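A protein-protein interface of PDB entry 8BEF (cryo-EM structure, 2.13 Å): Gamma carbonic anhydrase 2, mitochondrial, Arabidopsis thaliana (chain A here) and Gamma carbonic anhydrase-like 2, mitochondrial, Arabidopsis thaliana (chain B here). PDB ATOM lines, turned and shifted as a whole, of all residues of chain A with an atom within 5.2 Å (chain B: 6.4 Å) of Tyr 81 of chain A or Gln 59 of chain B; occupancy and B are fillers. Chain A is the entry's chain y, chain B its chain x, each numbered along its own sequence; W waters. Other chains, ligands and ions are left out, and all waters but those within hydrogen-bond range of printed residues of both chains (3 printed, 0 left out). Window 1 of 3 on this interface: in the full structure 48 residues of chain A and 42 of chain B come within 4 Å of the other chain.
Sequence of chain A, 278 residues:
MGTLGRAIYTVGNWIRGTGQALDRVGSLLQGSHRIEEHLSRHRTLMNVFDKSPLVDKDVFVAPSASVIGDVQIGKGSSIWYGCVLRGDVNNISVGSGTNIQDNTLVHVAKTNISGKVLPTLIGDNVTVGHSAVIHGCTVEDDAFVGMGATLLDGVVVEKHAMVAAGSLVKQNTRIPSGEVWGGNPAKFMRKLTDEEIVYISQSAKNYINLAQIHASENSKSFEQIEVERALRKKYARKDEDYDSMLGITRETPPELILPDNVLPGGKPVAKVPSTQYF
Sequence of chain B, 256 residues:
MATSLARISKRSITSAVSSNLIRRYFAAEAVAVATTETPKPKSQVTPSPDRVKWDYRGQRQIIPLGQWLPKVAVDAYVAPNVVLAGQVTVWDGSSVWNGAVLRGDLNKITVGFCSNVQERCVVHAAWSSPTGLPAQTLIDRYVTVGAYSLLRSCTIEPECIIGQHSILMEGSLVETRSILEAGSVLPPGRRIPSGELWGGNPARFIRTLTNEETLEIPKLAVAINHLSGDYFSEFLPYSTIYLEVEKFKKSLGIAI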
ATOM      1  N   PHE A  60     -24.922 -14.494  -4.294  1.00  0.00           N
ATOM      2  CA  PHE A  60     -25.589 -15.221  -3.223  1.00  0.00           C
ATOM      3  C   PHE A  60     -24.728 -16.412  -2.840  1.00  0.00           C
ATOM      4  O   PHE A  60     -24.473 -17.293  -3.666  1.00  0.00           O
ATOM      5  CB  PHE A  60     -26.986 -15.692  -3.629  1.00  0.00           C
ATOM      6  CG  PHE A  60     -27.646 -16.572  -2.594  1.00  0.00           C
ATOM      7  CD1 PHE A  60     -27.669 -16.196  -1.260  1.00  0.00           C
ATOM      8  CD2 PHE A  60     -28.226 -17.781  -2.951  1.00  0.00           C
ATOM      9  CE1 PHE A  60     -28.270 -16.996  -0.304  1.00  0.00           C
ATOM     10  CE2 PHE A  60     -28.827 -18.590  -1.997  1.00  0.00           C
ATOM     11  CZ  PHE A  60     -28.850 -18.199  -0.672  1.00  0.00           C
ATOM     12  N   ALA A  62     -25.192 -19.144   0.034  1.00  0.00           N
ATOM     13  CA  ALA A  62     -26.019 -19.623   1.125  1.00  0.00           C
ATOM     14  C   ALA A  62     -25.150 -19.830   2.363  1.00  0.00           C
ATOM     15  O   ALA A  62     -24.013 -20.297   2.250  1.00  0.00           O
ATOM     16  CB  ALA A  62     -26.720 -20.928   0.741  1.00  0.00           C
ATOM     17  N   PRO A  63     -25.640 -19.469   3.550  1.00  0.00           N
ATOM     18  CA  PRO A  63     -24.827 -19.644   4.765  1.00  0.00           C
ATOM     19  C   PRO A  63     -24.343 -21.070   4.972  1.00  0.00           C
ATOM     20  O   PRO A  63     -23.241 -21.269   5.495  1.00  0.00           O
ATOM     21  CB  PRO A  63     -25.780 -19.208   5.886  1.00  0.00           C
ATOM     22  CG  PRO A  63     -26.762 -18.298   5.224  1.00  0.00           C
ATOM     23  CD  PRO A  63     -26.920 -18.790   3.816  1.00  0.00           C
ATOM     24  N   SER A  64     -25.125 -22.068   4.566  1.00  0.00           N
ATOM     25  CA  SER A  64     -24.729 -23.463   4.716  1.00  0.00           C
ATOM     26  C   SER A  64     -23.748 -23.930   3.647  1.00  0.00           C
ATOM     27  O   SER A  64     -23.266 -25.063   3.731  1.00  0.00           O
ATOM     28  CB  SER A  64     -25.964 -24.365   4.698  1.00  0.00           C
ATOM     29  OG  SER A  64     -26.735 -24.153   3.533  1.00  0.00           O
ATOM     30  N   ALA A  65     -23.458 -23.105   2.645  1.00  0.00           N
ATOM     31  CA  ALA A  65     -22.465 -23.462   1.646  1.00  0.00           C
ATOM     32  C   ALA A  65     -21.057 -23.375   2.232  1.00  0.00           C
ATOM     33  O   ALA A  65     -20.803 -22.671   3.212  1.00  0.00           O
ATOM     34  CB  ALA A  65     -22.580 -22.557   0.419  1.00  0.00           C
ATOM     35  N   ILE A  79     -24.331 -19.551  -5.136  1.00  0.00           N
ATOM     36  CA  ILE A  79     -23.942 -20.822  -4.535  1.00  0.00           C
ATOM     37  C   ILE A  79     -25.016 -21.180  -3.518  1.00  0.00           C
ATOM     38  O   ILE A  79     -25.260 -20.422  -2.573  1.00  0.00           O
ATOM     39  CB  ILE A  79     -22.558 -20.741  -3.873  1.00  0.00           C
ATOM     40  CG1 ILE A  79     -21.537 -20.089  -4.811  1.00  0.00           C
ATOM     41  CG2 ILE A  79     -22.096 -22.119  -3.437  1.00  0.00           C
ATOM     42  CD1 ILE A  79     -21.340 -20.812  -6.116  1.00  0.00           C
ATOM     43  N   TRP A  80     -25.650 -22.331  -3.700  1.00  0.00           N
ATOM     44  CA  TRP A  80     -26.885 -22.629  -2.996  1.00  0.00           C
ATOM     45  C   TRP A  80     -26.620 -23.512  -1.774  1.00  0.00           C
ATOM     46  O   TRP A  80     -25.478 -23.799  -1.416  1.00  0.00           O
ATOM     47  CB  TRP A  80     -27.892 -23.235  -3.975  1.00  0.00           C
ATOM     48  CG  TRP A  80     -28.412 -22.174  -4.908  1.00  0.00           C
ATOM     49  CD1 TRP A  80     -27.813 -21.718  -6.047  1.00  0.00           C
ATOM     50  CD2 TRP A  80     -29.601 -21.395  -4.743  1.00  0.00           C
ATOM     51  NE1 TRP A  80     -28.569 -20.726  -6.616  1.00  0.00           N
ATOM     52  CE2 TRP A  80     -29.671 -20.504  -5.834  1.00  0.00           C
ATOM     53  CE3 TRP A  80     -30.621 -21.374  -3.788  1.00  0.00           C
ATOM     54  CZ2 TRP A  80     -30.719 -19.602  -5.994  1.00  0.00           C
ATOM     55  CZ3 TRP A  80     -31.662 -20.479  -3.950  1.00  0.00           C
ATOM     56  CH2 TRP A  80     -31.703 -19.605  -5.044  1.00  0.00           C
ATOM     57  N   TYR A  81     -27.704 -23.911  -1.106  1.00  0.00           N
ATOM     58  CA  TYR A  81     -27.612 -24.566   0.194  1.00  0.00           C
ATOM     59  C   TYR A  81     -26.855 -25.888   0.103  1.00  0.00           C
ATOM     60  O   TYR A  81     -27.135 -26.721  -0.761  1.00  0.00           O
ATOM     61  CB  TYR A  81     -29.017 -24.798   0.754  1.00  0.00           C
ATOM     62  CG  TYR A  81     -29.834 -23.529   0.851  1.00  0.00           C
ATOM     63  CD1 TYR A  81     -29.615 -22.615   1.873  1.00  0.00           C
ATOM     64  CD2 TYR A  81     -30.796 -23.229  -0.104  1.00  0.00           C
ATOM     65  CE1 TYR A  81     -30.350 -21.450   1.955  1.00  0.00           C
ATOM     66  CE2 TYR A  81     -31.533 -22.069  -0.033  1.00  0.00           C
ATOM     67  CZ  TYR A  81     -31.306 -21.182   0.998  1.00  0.00           C
ATOM     68  OH  TYR A  81     -32.039 -20.027   1.070  1.00  0.00           O
ATOM     69  N   GLY A  82     -25.891 -26.071   1.002  1.00  0.00           N
ATOM     70  CA  GLY A  82     -25.154 -27.313   1.097  1.00  0.00           C
ATOM     71  C   GLY A  82     -24.058 -27.503   0.071  1.00  0.00           C
ATOM     72  O   GLY A  82     -23.409 -28.555   0.078  1.00  0.00           O
ATOM     73  N   CYS A  83     -23.836 -26.536  -0.813  1.00  0.00           N
ATOM     74  CA  CYS A  83     -22.764 -26.645  -1.791  1.00  0.00           C
ATOM     75  C   CYS A  83     -21.399 -26.609  -1.113  1.00  0.00           C
ATOM     76  O   CYS A  83     -21.198 -25.929  -0.106  1.00  0.00           O
ATOM     77  CB  CYS A  83     -22.853 -25.513  -2.814  1.00  0.00           C
ATOM     78  SG  CYS A  83     -24.374 -25.465  -3.760  1.00  0.00           S
ATOM     79  N   GLN A 101     -26.174 -25.325  -7.959  1.00  0.00           N
ATOM     80  CA  GLN A 101     -27.369 -25.736  -7.178  1.00  0.00           C
ATOM     81  C   GLN A 101     -27.097 -26.510  -5.867  1.00  0.00           C
ATOM     82  O   GLN A 101     -26.019 -26.994  -5.704  1.00  0.00           O
ATOM     83  CB  GLN A 101     -28.399 -26.418  -8.049  1.00  0.00           C
ATOM     84  CG  GLN A 101     -29.063 -25.417  -8.999  1.00  0.00           C
ATOM     85  CD  GLN A 101     -29.929 -26.030 -10.073  1.00  0.00           C
ATOM     86  OE1 GLN A 101     -30.491 -27.100  -9.898  1.00  0.00           O
ATOM     87  NE2 GLN A 101     -30.052 -25.345 -11.198  1.00  0.00           N
ATOM     88  N   ASP A 102     -28.170 -26.777  -5.161  1.00  0.00           N
ATOM     89  CA  ASP A 102     -28.036 -27.267  -3.794  1.00  0.00           C
ATOM     90  C   ASP A 102     -27.291 -28.597  -3.735  1.00  0.00           C
ATOM     91  O   ASP A 102     -27.453 -29.460  -4.602  1.00  0.00           O
ATOM     92  CB  ASP A 102     -29.422 -27.430  -3.171  1.00  0.00           C
ATOM     93  CG  ASP A 102     -30.365 -26.295  -3.535  1.00  0.00           C
ATOM     94  OD1 ASP A 102     -30.839 -26.275  -4.688  1.00  0.00           O
ATOM     95  OD2 ASP A 102     -30.643 -25.440  -2.674  1.00  0.00           O
ATOM     96  N   ASN A 103     -26.466 -28.750  -2.699  1.00  0.00           N
ATOM     97  CA  ASN A 103     -25.782 -29.999  -2.363  1.00  0.00           C
ATOM     98  C   ASN A 103     -24.787 -30.436  -3.437  1.00  0.00           C
ATOM     99  O   ASN A 103     -24.456 -31.618  -3.531  1.00  0.00           O
ATOM    100  CB  ASN A 103     -26.789 -31.125  -2.086  1.00  0.00           C
ATOM    101  CG  ASN A 103     -27.376 -31.060  -0.681  1.00  0.00           C
ATOM    102  OD1 ASN A 103     -27.090 -30.143   0.083  1.00  0.00           O
ATOM    103  ND2 ASN A 103     -28.207 -32.038  -0.341  1.00  0.00           N
ATOM    104  N   HIS A 214     -33.380 -15.075  -2.186  1.00  0.00           N
ATOM    105  CA  HIS A 214     -32.746 -15.914  -1.166  1.00  0.00           C
ATOM    106  C   HIS A 214     -31.649 -15.159  -0.412  1.00  0.00           C
ATOM    107  O   HIS A 214     -31.542 -15.275   0.815  1.00  0.00           O
ATOM    108  CB  HIS A 214     -32.201 -17.198  -1.788  1.00  0.00           C
ATOM    109  CG  HIS A 214     -33.259 -18.218  -2.066  1.00  0.00           C
ATOM    110  ND1 HIS A 214     -33.572 -19.228  -1.182  1.00  0.00           N
ATOM    111  CD2 HIS A 214     -34.092 -18.371  -3.122  1.00  0.00           C
ATOM    112  CE1 HIS A 214     -34.543 -19.965  -1.687  1.00  0.00           C
ATOM    113  NE2 HIS A 214     -34.876 -19.468  -2.864  1.00  0.00           N
ATOM    114  N   ASN A 218     -31.623 -14.505   3.649  1.00  0.00           N
ATOM    115  CA  ASN A 218     -30.606 -15.125   4.496  1.00  0.00           C
ATOM    116  C   ASN A 218     -29.727 -14.108   5.218  1.00  0.00           C
ATOM    117  O   ASN A 218     -29.039 -14.476   6.174  1.00  0.00           O
ATOM    118  CB  ASN A 218     -29.731 -16.070   3.672  1.00  0.00           C
ATOM    119  CG  ASN A 218     -30.330 -17.461   3.544  1.00  0.00           C
ATOM    120  OD1 ASN A 218     -30.161 -18.305   4.420  1.00  0.00           O
ATOM    121  ND2 ASN A 218     -31.027 -17.704   2.443  1.00  0.00           N
ATOM    122  N   ASP B  55     -21.175 -16.880  10.165  1.00  0.00           N
ATOM    123  CA  ASP B  55     -22.447 -16.477  10.754  1.00  0.00           C
ATOM    124  C   ASP B  55     -22.661 -17.319  12.009  1.00  0.00           C
ATOM    125  O   ASP B  55     -22.833 -18.539  11.922  1.00  0.00           O
ATOM    126  CB  ASP B  55     -23.583 -16.661   9.747  1.00  0.00           C
ATOM    127  CG  ASP B  55     -24.897 -16.050  10.209  1.00  0.00           C
ATOM    128  OD1 ASP B  55     -25.172 -16.030  11.425  1.00  0.00           O
ATOM    129  OD2 ASP B  55     -25.673 -15.605   9.343  1.00  0.00           O
ATOM    130  N   ARG B  57     -25.102 -17.758  13.836  1.00  0.00           N
ATOM    131  CA  ARG B  57     -26.397 -18.412  13.955  1.00  0.00           C
ATOM    132  C   ARG B  57     -26.477 -19.715  13.173  1.00  0.00           C
ATOM    133  O   ARG B  57     -27.383 -20.515  13.424  1.00  0.00           O
ATOM    134  CB  ARG B  57     -27.503 -17.464  13.491  1.00  0.00           C
ATOM    135  CG  ARG B  57     -27.359 -16.048  14.025  1.00  0.00           C
ATOM    136  CD  ARG B  57     -28.213 -15.065  13.249  1.00  0.00           C
ATOM    137  NE  ARG B  57     -27.668 -14.747  11.933  1.00  0.00           N
ATOM    138  CZ  ARG B  57     -28.245 -13.918  11.071  1.00  0.00           C
ATOM    139  NH1 ARG B  57     -29.374 -13.294  11.364  1.00  0.00           N
ATOM    140  NH2 ARG B  57     -27.677 -13.715   9.887  1.00  0.00           N
ATOM    141  N   GLY B  58     -25.550 -19.954  12.252  1.00  0.00           N
ATOM    142  CA  GLY B  58     -25.665 -21.078  11.348  1.00  0.00           C
ATOM    143  C   GLY B  58     -26.759 -20.831  10.320  1.00  0.00           C
ATOM    144  O   GLY B  58     -27.377 -19.774  10.261  1.00  0.00           O
ATOM    145  N   GLN B  59     -26.999 -21.845   9.500  1.00  0.00           N
ATOM    146  CA  GLN B  59     -28.034 -21.760   8.479  1.00  0.00           C
ATOM    147  C   GLN B  59     -29.404 -21.905   9.130  1.00  0.00           C
ATOM    148  O   GLN B  59     -29.660 -22.893   9.825  1.00  0.00           O
ATOM    149  CB  GLN B  59     -27.822 -22.837   7.418  1.00  0.00           C
ATOM    150  CG  GLN B  59     -29.003 -23.022   6.484  1.00  0.00           C
ATOM    151  CD  GLN B  59     -29.182 -21.855   5.530  1.00  0.00           C
ATOM    152  OE1 GLN B  59     -28.293 -21.549   4.740  1.00  0.00           O
ATOM    153  NE2 GLN B  59     -30.332 -21.200   5.600  1.00  0.00           N
ATOM    154  N   ARG B  60     -30.279 -20.927   8.910  1.00  0.00           N
ATOM    155  CA  ARG B  60     -31.649 -21.037   9.396  1.00  0.00           C
ATOM    156  C   ARG B  60     -32.357 -22.207   8.726  1.00  0.00           C
ATOM    157  O   ARG B  60     -32.274 -22.386   7.508  1.00  0.00           O
ATOM    158  CB  ARG B  60     -32.419 -19.743   9.138  1.00  0.00           C
ATOM    159  CG  ARG B  60     -32.713 -18.939  10.392  1.00  0.00           C
ATOM    160  CD  ARG B  60     -33.718 -17.827  10.138  1.00  0.00           C
ATOM    161  NE  ARG B  60     -33.231 -16.852   9.171  1.00  0.00           N
ATOM    162  CZ  ARG B  60     -34.013 -16.141   8.370  1.00  0.00           C
ATOM    163  NH1 ARG B  60     -35.327 -16.271   8.396  1.00  0.00           N
ATOM    164  NH2 ARG B  60     -33.460 -15.280   7.522  1.00  0.00           N
ATOM    165  N   GLN B  61     -33.059 -23.005   9.533  1.00  0.00           N
ATOM    166  CA  GLN B  61     -33.775 -24.156   8.995  1.00  0.00           C
ATOM    167  C   GLN B  61     -34.989 -23.731   8.175  1.00  0.00           C
ATOM    168  O   GLN B  61     -35.276 -24.324   7.129  1.00  0.00           O
ATOM    169  CB  GLN B  61     -34.197 -25.087  10.132  1.00  0.00           C
ATOM    170  CG  GLN B  61     -34.930 -26.330   9.670  1.00  0.00           C
ATOM    171  CD  GLN B  61     -35.357 -27.224  10.817  1.00  0.00           C
ATOM    172  OE1 GLN B  61     -36.373 -26.982  11.461  1.00  0.00           O
ATOM    173  NE2 GLN B  61     -34.581 -28.268  11.073  1.00  0.00           N
ATOM    174  N   ILE B  62     -35.712 -22.715   8.632  1.00  0.00           N
ATOM    175  CA  ILE B  62     -36.950 -22.271   8.000  1.00  0.00           C
ATOM    176  C   ILE B  62     -36.649 -20.975   7.261  1.00  0.00           C
ATOM    177  O   ILE B  62     -36.362 -19.946   7.883  1.00  0.00           O
ATOM    178  CB  ILE B  62     -38.077 -22.074   9.024  1.00  0.00           C
ATOM    179  CG1 ILE B  62     -38.380 -23.386   9.753  1.00  0.00           C
ATOM    180  CG2 ILE B  62     -39.324 -21.519   8.344  1.00  0.00           C
ATOM    181  CD1 ILE B  62     -38.878 -24.477   8.857  1.00  0.00           C
ATOM    182  N   ILE B  63     -36.730 -21.016   5.937  1.00  0.00           N
ATOM    183  CA  ILE B  63     -36.476 -19.835   5.119  1.00  0.00           C
ATOM    184  C   ILE B  63     -37.801 -19.347   4.545  1.00  0.00           C
ATOM    185  O   ILE B  63     -38.324 -19.948   3.598  1.00  0.00           O
ATOM    186  CB  ILE B  63     -35.460 -20.134   4.004  1.00  0.00           C
ATOM    187  CG1 ILE B  63     -34.099 -20.506   4.603  1.00  0.00           C
ATOM    188  CG2 ILE B  63     -35.335 -18.947   3.056  1.00  0.00           C
ATOM    189  CD1 ILE B  63     -33.436 -19.381   5.358  1.00  0.00           C
ATOM    190  N   LEU B  65     -40.168 -16.824   2.307  1.00  0.00           N
ATOM    191  CA  LEU B  65     -39.966 -16.145   1.024  1.00  0.00           C
ATOM    192  C   LEU B  65     -41.203 -15.280   0.789  1.00  0.00           C
ATOM    193  O   LEU B  65     -42.204 -15.745   0.242  1.00  0.00           O
ATOM    194  CB  LEU B  65     -39.745 -17.150  -0.099  1.00  0.00           C
ATOM    195  CG  LEU B  65     -38.393 -17.876  -0.124  1.00  0.00           C
ATOM    196  CD1 LEU B  65     -38.287 -18.783  -1.336  1.00  0.00           C
ATOM    197  CD2 LEU B  65     -37.235 -16.895  -0.092  1.00  0.00           C
ATOM    198  N   PRO B  80     -32.111 -31.091  12.220  1.00  0.00           N
ATOM    199  CA  PRO B  80     -31.696 -29.695  12.464  1.00  0.00           C
ATOM    200  C   PRO B  80     -31.055 -29.004  11.269  1.00  0.00           C
ATOM    201  O   PRO B  80     -31.265 -27.799  11.090  1.00  0.00           O
ATOM    202  CB  PRO B  80     -30.710 -29.830  13.634  1.00  0.00           C
ATOM    203  CG  PRO B  80     -31.099 -31.096  14.307  1.00  0.00           C
ATOM    204  CD  PRO B  80     -31.534 -32.016  13.212  1.00  0.00           C
ATOM    205  N   ASN B  81     -30.287 -29.713  10.444  1.00  0.00           N
ATOM    206  CA  ASN B  81     -29.569 -29.068   9.350  1.00  0.00           C
ATOM    207  C   ASN B  81     -30.330 -29.106   8.026  1.00  0.00           C
ATOM    208  O   ASN B  81     -29.774 -28.714   6.997  1.00  0.00           O
ATOM    209  CB  ASN B  81     -28.173 -29.684   9.189  1.00  0.00           C
ATOM    210  CG  ASN B  81     -28.207 -31.110   8.674  1.00  0.00           C
ATOM    211  OD1 ASN B  81     -29.207 -31.809   8.798  1.00  0.00           O
ATOM    212  ND2 ASN B  81     -27.092 -31.554   8.113  1.00  0.00           N
ATOM    213  N   VAL B  82     -31.583 -29.563   8.035  1.00  0.00           N
ATOM    214  CA  VAL B  82     -32.430 -29.485   6.850  1.00  0.00           C
ATOM    215  C   VAL B  82     -32.755 -28.024   6.547  1.00  0.00           C
ATOM    216  O   VAL B  82     -32.873 -27.190   7.453  1.00  0.00           O
ATOM    217  CB  VAL B  82     -33.714 -30.312   7.068  1.00  0.00           C
ATOM    218  CG1 VAL B  82     -34.742 -30.050   5.972  1.00  0.00           C
ATOM    219  CG2 VAL B  82     -33.388 -31.792   7.159  1.00  0.00           C
ATOM    220  N   VAL B  83     -32.895 -27.703   5.265  1.00  0.00           N
ATOM    221  CA  VAL B  83     -33.348 -26.386   4.828  1.00  0.00           C
ATOM    222  C   VAL B  83     -34.709 -26.544   4.163  1.00  0.00           C
ATOM    223  O   VAL B  83     -34.859 -27.318   3.212  1.00  0.00           O
ATOM    224  CB  VAL B  83     -32.342 -25.725   3.875  1.00  0.00           C
ATOM    225  CG1 VAL B  83     -32.928 -24.446   3.290  1.00  0.00           C
ATOM    226  CG2 VAL B  83     -31.033 -25.441   4.597  1.00  0.00           C
ATOM    227  N   ALA B  85     -37.502 -24.023   2.378  1.00  0.00           N
ATOM    228  CA  ALA B  85     -37.636 -22.665   1.865  1.00  0.00           C
ATOM    229  C   ALA B  85     -38.925 -22.519   1.070  1.00  0.00           C
ATOM    230  O   ALA B  85     -39.211 -23.333   0.188  1.00  0.00           O
ATOM    231  CB  ALA B  85     -36.432 -22.286   0.999  1.00  0.00           C
ATOM    232  N   VAL B 101     -32.671 -30.860   1.384  1.00  0.00           N
ATOM    233  CA  VAL B 101     -33.033 -29.502   0.996  1.00  0.00           C
ATOM    234  C   VAL B 101     -34.369 -29.562   0.270  1.00  0.00           C
ATOM    235  O   VAL B 101     -34.509 -30.288  -0.721  1.00  0.00           O
ATOM    236  CB  VAL B 101     -31.962 -28.850   0.105  1.00  0.00           C
ATOM    237  CG1 VAL B 101     -32.414 -27.462  -0.357  1.00  0.00           C
ATOM    238  CG2 VAL B 101     -30.631 -28.773   0.836  1.00  0.00           C
ATOM    239  N   ARG B 103     -36.840 -26.914  -1.491  1.00  0.00           N
ATOM    240  CA  ARG B 103     -36.884 -25.527  -1.949  1.00  0.00           C
ATOM    241  C   ARG B 103     -38.151 -25.311  -2.773  1.00  0.00           C
ATOM    242  O   ARG B 103     -38.207 -25.680  -3.948  1.00  0.00           O
ATOM    243  CB  ARG B 103     -35.631 -25.184  -2.748  1.00  0.00           C
ATOM    244  CG  ARG B 103     -35.506 -23.711  -3.093  1.00  0.00           C
ATOM    245  CD  ARG B 103     -34.057 -23.251  -3.072  1.00  0.00           C
ATOM    246  NE  ARG B 103     -33.220 -24.018  -3.986  1.00  0.00           N
ATOM    247  CZ  ARG B 103     -33.073 -23.745  -5.274  1.00  0.00           C
ATOM    248  NH1 ARG B 103     -33.704 -22.730  -5.842  1.00  0.00           N
ATOM    249  NH2 ARG B 103     -32.276 -24.510  -6.013  1.00  0.00           N
HETATM  250  O   HOH W   1     -24.109 -21.077   8.064  1.00  0.00           O
HETATM  251  O   HOH W   2     -30.787 -14.234   8.393  1.00  0.00           O
HETATM  252  O   HOH W   3     -29.820 -18.518   7.436  1.00  0.00           O
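NE2 of Gln 59 of chain B is in hydrogen-bond range of OD1 of Asn 218 of chain A.
OE1 of Gln 59 of chain B lies within hydrogen-bond range of N of Ser 64 of chain A, at 3.2 Å.
The guanidinium group of Arg 103 of chain B lies within salt-bridge range of the side-chain carboxylate of Asp 102 of chain A (2.6 Å).
O of His 214 of chain A lies within hydrogen-bond range of ND2 of Asn 218 of chain A.
OG of Ser 64 of chain A sits at hydrogen-bond distance from N of Gly 82 of chain A.
The backbone carbonyl oxygen (O) of Tyr 81 of chain A is in hydrogen-bond range of the backbone NH (N) of Asn 103 of chain A.
The side-chain hydroxyl (OH) of Tyr 81 of chain A lies within hydrogen-bond range of a ring nitrogen (ND1) of His 214 of chain A (2.8 Å).
The side-chain amide nitrogen (ND2) of Asn 218 of chain A sits at hydrogen-bond distance from the side-chain hydroxyl (OH) of Tyr 81 of chain A (2.9 Å).
SG of Cys 83 of chain A lies within hydrogen-bond range of O of Trp 80 of chain A (3.1 Å).
CD of Pro 63 of chain A touches OE1 of Gln 59 of chain B, at 3.2 Å.
Arg 103 of chain B touches Trp 80 of chain A.
Tyr 81 of chain A touches Gln 59 of chain B (CD1 to OE1, 3.3 Å).
CG2 of Ile 63 of chain B touches OH of Tyr 81 of chain A (3.997 Å).
OD2 of Asp 102 of chain A touches CG1 of Val 101 of chain B, at 3.5 Å.
Asn 103 of chain A touches Val 101 of chain B.
Leu 65 of chain B touches His 214 of chain A (CD1 to NE2, 3.8 Å).
His 214 of chain A touches Arg 103 of chain B.
OD1 of Asn 218 of chain A touches CD1 of Ile 63 of chain B, 3.6 Å away.
Printed residues of chain B within 4 Å of Tyr 81 of chain A: Gln 59 (3.3 Å) and Ile 63 (3.997 Å).
Of the printed residues of chain A, Gln 59 of chain B touches Pro 63 (3.2 Å), Ser 64 (3.2 Å), Tyr 81 (3.3 Å) and Asn 218 (3.1 Å).
Of the printed residues of chain B, Trp 80 of chain A touches Arg 103 (3.6 Å).
Of the printed residues of chain A, Ile 63 of chain B touches Tyr 81 and Asn 218.
Of the printed residues of chain B, His 214 of chain A touches Leu 65 and Arg 103.
Printed residues of chain B within 4 Å of Asp 102 of chain A: Val 101 (3.5 Å) and Arg 103 (2.6 Å).
Of the printed residues of chain A, Val 101 of chain B touches Asp 102 (3.5 Å) and Asn 103 (3.9 Å).
Asp 55 of chain B touches none of the printed residues of chain A.
The nearest printed residue of chain B that does not touch Tyr 81 of chain A is Val 83 of chain B (4.04 Å).
The nearest residue of chain A that does not touch Gln 59 of chain B is Ala 62 of chain A (4.3 Å).
The nearest printed residue of chain B that does not touch Asn 218 of chain A is Arg 57 of chain B (4.03 Å).
Of the 15 printed residues of chain A, 8 touch a printed residue of chain B.
Printed residues of chain A that touch a printed residue of chain B: Pro 63, Ser 64, Trp 80, Tyr 81, Asp 102, Asn 103, His 214 and Asn 218.
Hydrophobic or aromatic side chains of chain A within 4 Å of the printed part of chain B: Pro 63, Trp 80, Tyr 81 and His 214.
Of the 16 printed residues of chain B, 5 touch a printed residue of chain A.
Printed residues of chain B that touch a printed residue of chain A: Gln 59, Ile 63, Leu 65, Val 101 and Arg 103.
Hydrophobic or aromatic side chains of chain B that line the printed part of chain A: Ile 63, Leu 65 and Val 101.
Water W1 bridges O of Pro 63 of chain A (2.7 Å) and N of Gln 59 of chain B (3.3 Å).
Water W2 lies within hydrogen-bond range of the backbone carbonyl oxygen of Asn 218 of chain A (2.8 Å), the guanidinium group of Arg 60 of chain B (3.0 Å) and the guanidinium group of Arg 57 of chain B (3.4 Å).
Water W3 lies within hydrogen-bond range of N of Arg 60 of chain B (2.9 Å), OD1 of Asn 218 of chain A (3.0 Å) and NE2 of Gln 59 of chain B (3.3 Å).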
